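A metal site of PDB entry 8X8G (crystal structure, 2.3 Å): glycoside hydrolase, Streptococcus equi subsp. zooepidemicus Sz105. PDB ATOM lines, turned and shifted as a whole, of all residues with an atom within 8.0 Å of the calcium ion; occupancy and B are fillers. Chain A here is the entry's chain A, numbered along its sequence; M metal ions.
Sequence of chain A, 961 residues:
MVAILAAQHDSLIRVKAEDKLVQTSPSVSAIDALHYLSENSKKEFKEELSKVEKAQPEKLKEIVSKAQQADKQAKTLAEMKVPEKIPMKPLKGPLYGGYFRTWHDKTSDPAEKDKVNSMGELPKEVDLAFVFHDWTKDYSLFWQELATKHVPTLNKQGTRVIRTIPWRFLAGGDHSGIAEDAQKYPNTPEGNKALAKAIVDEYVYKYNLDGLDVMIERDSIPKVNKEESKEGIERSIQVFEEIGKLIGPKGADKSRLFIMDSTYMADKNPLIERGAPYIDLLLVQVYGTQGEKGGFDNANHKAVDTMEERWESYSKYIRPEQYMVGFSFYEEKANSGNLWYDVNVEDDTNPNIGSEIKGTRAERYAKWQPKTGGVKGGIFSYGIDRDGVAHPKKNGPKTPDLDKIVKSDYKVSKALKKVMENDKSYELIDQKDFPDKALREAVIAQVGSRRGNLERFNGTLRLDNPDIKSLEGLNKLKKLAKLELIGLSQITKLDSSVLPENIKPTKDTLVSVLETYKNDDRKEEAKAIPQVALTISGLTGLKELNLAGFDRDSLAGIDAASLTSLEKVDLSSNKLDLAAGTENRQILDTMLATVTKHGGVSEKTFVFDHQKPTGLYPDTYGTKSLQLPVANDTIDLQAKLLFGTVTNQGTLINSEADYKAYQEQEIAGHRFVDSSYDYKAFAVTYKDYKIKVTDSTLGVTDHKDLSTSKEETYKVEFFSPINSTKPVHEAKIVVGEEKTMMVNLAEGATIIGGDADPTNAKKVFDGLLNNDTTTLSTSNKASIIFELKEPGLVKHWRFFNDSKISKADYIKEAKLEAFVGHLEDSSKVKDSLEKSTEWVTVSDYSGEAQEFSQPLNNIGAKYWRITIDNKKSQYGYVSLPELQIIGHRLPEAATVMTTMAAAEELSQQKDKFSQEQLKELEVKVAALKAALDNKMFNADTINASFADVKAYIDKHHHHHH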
ATOM      1  N   ASN A 760       4.546  -4.169 -29.526  1.00  0.00           N
ATOM      2  CA  ASN A 760       4.496  -5.202 -28.498  1.00  0.00           C
ATOM      3  C   ASN A 760       4.707  -4.636 -27.108  1.00  0.00           C
ATOM      4  O   ASN A 760       4.263  -5.237 -26.118  1.00  0.00           O
ATOM      5  CB  ASN A 760       5.540  -6.278 -28.802  1.00  0.00           C
ATOM      6  CG  ASN A 760       5.221  -7.048 -30.079  1.00  0.00           C
ATOM      7  OD1 ASN A 760       4.206  -6.800 -30.729  1.00  0.00           O
ATOM      8  ND2 ASN A 760       6.091  -7.984 -30.439  1.00  0.00           N
ATOM      9  N   ALA A 761       5.386  -3.487 -26.989  1.00  0.00           N
ATOM     10  CA  ALA A 761       5.537  -2.846 -25.685  1.00  0.00           C
ATOM     11  C   ALA A 761       4.182  -2.436 -25.117  1.00  0.00           C
ATOM     12  O   ALA A 761       3.950  -2.563 -23.908  1.00  0.00           O
ATOM     13  CB  ALA A 761       6.451  -1.630 -25.797  1.00  0.00           C
ATOM     14  N   LYS A 762       3.280  -1.943 -25.976  1.00  0.00           N
ATOM     15  CA  LYS A 762       1.931  -1.611 -25.519  1.00  0.00           C
ATOM     16  C   LYS A 762       1.222  -2.849 -24.981  1.00  0.00           C
ATOM     17  O   LYS A 762       0.443  -2.758 -24.026  1.00  0.00           O
ATOM     18  CB  LYS A 762       1.139  -0.991 -26.674  1.00  0.00           C
ATOM     19  CG  LYS A 762       1.212   0.523 -26.739  1.00  0.00           C
ATOM     20  CD  LYS A 762       0.462   1.054 -27.944  1.00  0.00           C
ATOM     21  CE  LYS A 762       1.104   2.313 -28.498  1.00  0.00           C
ATOM     22  NZ  LYS A 762       1.060   2.366 -29.988  1.00  0.00           N
ATOM     23  N   LYS A 763       1.470  -4.010 -25.585  1.00  0.00           N
ATOM     24  CA  LYS A 763       0.840  -5.255 -25.164  1.00  0.00           C
ATOM     25  C   LYS A 763       1.329  -5.741 -23.811  1.00  0.00           C
ATOM     26  O   LYS A 763       0.734  -6.669 -23.256  1.00  0.00           O
ATOM     27  CB  LYS A 763       1.066  -6.325 -26.239  1.00  0.00           C
ATOM     28  CG  LYS A 763       0.678  -5.871 -27.629  1.00  0.00           C
ATOM     29  CD  LYS A 763       0.447  -7.031 -28.574  1.00  0.00           C
ATOM     30  CE  LYS A 763       1.726  -7.818 -28.812  1.00  0.00           C
ATOM     31  NZ  LYS A 763       1.789  -8.339 -30.196  1.00  0.00           N
ATOM     32  N   VAL A 764       2.393  -5.144 -23.267  1.00  0.00           N
ATOM     33  CA  VAL A 764       2.852  -5.478 -21.932  1.00  0.00           C
ATOM     34  C   VAL A 764       1.877  -4.978 -20.860  1.00  0.00           C
ATOM     35  O   VAL A 764       1.865  -5.505 -19.744  1.00  0.00           O
ATOM     36  CB  VAL A 764       4.270  -4.920 -21.714  1.00  0.00           C
ATOM     37  CG1 VAL A 764       4.772  -5.173 -20.300  1.00  0.00           C
ATOM     38  CG2 VAL A 764       5.233  -5.507 -22.734  1.00  0.00           C
ATOM     39  N   PHE A 765       1.051  -3.986 -21.190  1.00  0.00           N
ATOM     40  CA  PHE A 765       0.193  -3.347 -20.198  1.00  0.00           C
ATOM     41  C   PHE A 765      -1.293  -3.407 -20.575  1.00  0.00           C
ATOM     42  O   PHE A 765      -2.096  -2.656 -20.021  1.00  0.00           O
ATOM     43  CB  PHE A 765       0.630  -1.904 -19.985  1.00  0.00           C
ATOM     44  CG  PHE A 765       2.081  -1.762 -19.596  1.00  0.00           C
ATOM     45  CD1 PHE A 765       2.510  -2.137 -18.333  1.00  0.00           C
ATOM     46  CD2 PHE A 765       3.014  -1.257 -20.485  1.00  0.00           C
ATOM     47  CE1 PHE A 765       3.830  -2.015 -17.966  1.00  0.00           C
ATOM     48  CE2 PHE A 765       4.344  -1.142 -20.126  1.00  0.00           C
ATOM     49  CZ  PHE A 765       4.751  -1.514 -18.868  1.00  0.00           C
ATOM     50  N   ASP A 766      -1.666  -4.291 -21.507  1.00  0.00           N
ATOM     51  CA  ASP A 766      -3.067  -4.359 -21.939  1.00  0.00           C
ATOM     52  C   ASP A 766      -3.938  -5.108 -20.928  1.00  0.00           C
ATOM     53  O   ASP A 766      -5.076  -4.704 -20.688  1.00  0.00           O
ATOM     54  CB  ASP A 766      -3.163  -4.991 -23.327  1.00  0.00           C
ATOM     55  CG  ASP A 766      -2.644  -6.422 -23.362  1.00  0.00           C
ATOM     56  OD1 ASP A 766      -2.017  -6.861 -22.370  1.00  0.00           O
ATOM     57  OD2 ASP A 766      -2.863  -7.097 -24.387  1.00  0.00           O
ATOM     58  N   GLY A 767      -3.428  -6.186 -20.349  1.00  0.00           N
ATOM     59  CA  GLY A 767      -4.174  -6.910 -19.328  1.00  0.00           C
ATOM     60  C   GLY A 767      -4.215  -8.414 -19.515  1.00  0.00           C
ATOM     61  O   GLY A 767      -4.770  -9.136 -18.674  1.00  0.00           O
ATOM     62  N   LEU A 768      -3.628  -8.908 -20.604  1.00  0.00           N
ATOM     63  CA  LEU A 768      -3.731 -10.313 -20.983  1.00  0.00           C
ATOM     64  C   LEU A 768      -2.486 -11.042 -20.516  1.00  0.00           C
ATOM     65  O   LEU A 768      -1.379 -10.718 -20.942  1.00  0.00           O
ATOM     66  CB  LEU A 768      -3.891 -10.446 -22.498  1.00  0.00           C
ATOM     67  CG  LEU A 768      -5.235 -10.196 -23.203  1.00  0.00           C
ATOM     68  CD1 LEU A 768      -6.318 -11.173 -22.736  1.00  0.00           C
ATOM     69  CD2 LEU A 768      -5.691  -8.746 -23.044  1.00  0.00           C
ATOM     70  N   LEU A 769      -2.662 -12.029 -19.632  1.00  0.00           N
ATOM     71  CA  LEU A 769      -1.497 -12.703 -19.065  1.00  0.00           C
ATOM     72  C   LEU A 769      -0.965 -13.760 -20.019  1.00  0.00           C
ATOM     73  O   LEU A 769       0.202 -14.154 -19.915  1.00  0.00           O
ATOM     74  CB  LEU A 769      -1.850 -13.348 -17.731  1.00  0.00           C
ATOM     75  CG  LEU A 769      -2.063 -12.381 -16.556  1.00  0.00           C
ATOM     76  CD1 LEU A 769      -0.895 -11.439 -16.383  1.00  0.00           C
ATOM     77  CD2 LEU A 769      -3.399 -11.644 -16.610  1.00  0.00           C
ATOM     78  N   ASN A 770      -1.819 -14.238 -20.920  1.00  0.00           N
ATOM     79  CA  ASN A 770      -1.465 -15.141 -22.014  1.00  0.00           C
ATOM     80  C   ASN A 770      -1.543 -14.400 -23.344  1.00  0.00           C
ATOM     81  O   ASN A 770      -2.069 -14.906 -24.331  1.00  0.00           O
ATOM     82  CB  ASN A 770      -2.373 -16.363 -22.023  1.00  0.00           C
ATOM     83  CG  ASN A 770      -1.751 -17.550 -21.313  1.00  0.00           C
ATOM     84  OD1 ASN A 770      -0.687 -18.015 -21.693  1.00  0.00           O
ATOM     85  ND2 ASN A 770      -2.406 -18.034 -20.268  1.00  0.00           N
ATOM     86  N   ASN A 771      -1.039 -13.162 -23.356  1.00  0.00           N
ATOM     87  CA  ASN A 771      -1.081 -12.298 -24.533  1.00  0.00           C
ATOM     88  C   ASN A 771      -0.029 -12.729 -25.548  1.00  0.00           C
ATOM     89  O   ASN A 771       0.856 -11.955 -25.921  1.00  0.00           O
ATOM     90  CB  ASN A 771      -0.890 -10.854 -24.111  1.00  0.00           C
ATOM     91  CG  ASN A 771      -1.235  -9.871 -25.210  1.00  0.00           C
ATOM     92  OD1 ASN A 771      -1.646 -10.252 -26.306  1.00  0.00           O
ATOM     93  ND2 ASN A 771      -1.045  -8.586 -24.931  1.00  0.00           N
ATOM     94  N   ASP A 772      -0.131 -13.979 -26.002  1.00  0.00           N
ATOM     95  CA  ASP A 772       0.716 -14.407 -27.110  1.00  0.00           C
ATOM     96  C   ASP A 772       0.074 -14.011 -28.439  1.00  0.00           C
ATOM     97  O   ASP A 772      -0.267 -14.830 -29.291  1.00  0.00           O
ATOM     98  CB  ASP A 772       1.028 -15.890 -27.065  1.00  0.00           C
ATOM     99  CG  ASP A 772       2.294 -16.232 -27.846  1.00  0.00           C
ATOM    100  OD1 ASP A 772       2.341 -15.958 -29.062  1.00  0.00           O
ATOM    101  OD2 ASP A 772       3.266 -16.728 -27.231  1.00  0.00           O
ATOM    102  N   THR A 773      -0.089 -12.701 -28.582  1.00  0.00           N
ATOM    103  CA  THR A 773      -0.093 -12.032 -29.867  1.00  0.00           C
ATOM    104  C   THR A 773       1.319 -11.624 -30.256  1.00  0.00           C
ATOM    105  O   THR A 773       1.503 -10.565 -30.881  1.00  0.00           O
ATOM    106  CB  THR A 773      -1.033 -10.838 -29.858  1.00  0.00           C
ATOM    107  OG1 THR A 773      -0.711  -9.978 -28.768  1.00  0.00           O
ATOM    108  CG2 THR A 773      -2.480 -11.300 -29.726  1.00  0.00           C
ATOM    109  N   THR A 775       4.378 -11.130 -27.911  1.00  0.00           N
ATOM    110  CA  THR A 775       4.760 -10.094 -26.959  1.00  0.00           C
ATOM    111  C   THR A 775       6.281  -9.871 -26.877  1.00  0.00           C
ATOM    112  O   THR A 775       6.764  -9.408 -25.841  1.00  0.00           O
ATOM    113  CB  THR A 775       4.222 -10.435 -25.573  1.00  0.00           C
ATOM    114  OG1 THR A 775       4.523  -9.371 -24.662  1.00  0.00           O
ATOM    115  CG2 THR A 775       4.850 -11.737 -25.061  1.00  0.00           C
ATOM    116  N   LEU A 880       7.910 -10.372 -23.103  1.00  0.00           N
ATOM    117  CA  LEU A 880       7.317  -9.919 -21.835  1.00  0.00           C
ATOM    118  C   LEU A 880       5.798  -9.820 -21.995  1.00  0.00           C
ATOM    119  O   LEU A 880       5.272  -8.801 -22.445  1.00  0.00           O
ATOM    120  CB  LEU A 880       7.892  -8.576 -21.394  1.00  0.00           C
ATOM    121  CG  LEU A 880       7.425  -8.014 -20.056  1.00  0.00           C
ATOM    122  CD1 LEU A 880       7.542  -9.062 -18.961  1.00  0.00           C
ATOM    123  CD2 LEU A 880       8.218  -6.770 -19.692  1.00  0.00           C
ATOM    124  N   PRO A 881       5.068 -10.890 -21.641  1.00  0.00           N
ATOM    125  CA  PRO A 881       3.602 -10.887 -21.818  1.00  0.00           C
ATOM    126  C   PRO A 881       2.842  -9.848 -20.968  1.00  0.00           C
ATOM    127  O   PRO A 881       1.995  -9.134 -21.519  1.00  0.00           O
ATOM    128  CB  PRO A 881       3.191 -12.315 -21.461  1.00  0.00           C
ATOM    129  CG  PRO A 881       4.409 -12.963 -20.846  1.00  0.00           C
ATOM    130  CD  PRO A 881       5.582 -12.253 -21.420  1.00  0.00           C
ATOM    131  N   GLU A 882       3.084  -9.772 -19.654  1.00  0.00           N
ATOM    132  CA  GLU A 882       2.565  -8.655 -18.861  1.00  0.00           C
ATOM    133  C   GLU A 882       3.622  -8.203 -17.864  1.00  0.00           C
ATOM    134  O   GLU A 882       4.479  -8.961 -17.408  1.00  0.00           O
ATOM    135  CB  GLU A 882       1.281  -8.962 -18.050  1.00  0.00           C
ATOM    136  CG  GLU A 882      -0.095  -8.859 -18.728  1.00  0.00           C
ATOM    137  CD  GLU A 882      -0.438  -7.446 -19.201  1.00  0.00           C
ATOM    138  OE1 GLU A 882      -1.164  -6.685 -18.509  1.00  0.00           O
ATOM    139  OE2 GLU A 882      -0.096  -7.128 -20.354  1.00  0.00           O
ATOM    140  N   LEU A 883       3.537  -6.914 -17.526  1.00  0.00           N
ATOM    141  CA  LEU A 883       4.163  -6.351 -16.332  1.00  0.00           C
ATOM    142  C   LEU A 883       3.091  -5.621 -15.539  1.00  0.00           C
ATOM    143  O   LEU A 883       2.262  -4.907 -16.108  1.00  0.00           O
ATOM    144  CB  LEU A 883       5.301  -5.397 -16.701  1.00  0.00           C
ATOM    145  CG  LEU A 883       5.996  -4.689 -15.536  1.00  0.00           C
ATOM    146  CD1 LEU A 883       6.963  -5.625 -14.846  1.00  0.00           C
ATOM    147  CD2 LEU A 883       6.719  -3.448 -16.030  1.00  0.00           C
HETATM  148 CA    CA M   1      -0.263  -8.863 -22.304  1.00  0.00          CA
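The side-chain amino group of Lys 763 sits close to the side-chain hydroxyl of Thr 773, at 3.3 Å. The side-chain amino group (NZ) of Lys 763 is in hydrogen-bond range of the side-chain amide oxygen (OD1) of Asn 760, 2.9 Å away. N of Gly 767 lies within hydrogen-bond range of OE1 of Glu 882, at 3.0 Å. The side-chain carboxylate of Glu 882 lies close to the backbone carbonyl oxygen of Val 764 (2.6 Å). The side-chain carboxylate (OE2) of Glu 882 sits close to the backbone NH (N) of Phe 765 (3.4 Å). The side-chain amide oxygen (OD1) of Asn 771 sits at hydrogen-bond distance from the side-chain hydroxyl (OG1) of Thr 773 (2.6 Å).
The calcium ion is bound by the backbone carbonyl oxygen (O) of Pro 881. The backbone carbonyl oxygen (O) of Leu 768 binds the calcium ion (2.6 Å). O of Lys 763 binds the calcium ion, at 2.6 Å. The side-chain carboxylate (OE2) of Glu 882 is bound to the calcium ion (2.6 Å). The calcium ion is bound by OD1 of Asp 766 (2.7 Å). ND2 of Asn 771 is bound to the calcium ion (2.8 Å).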
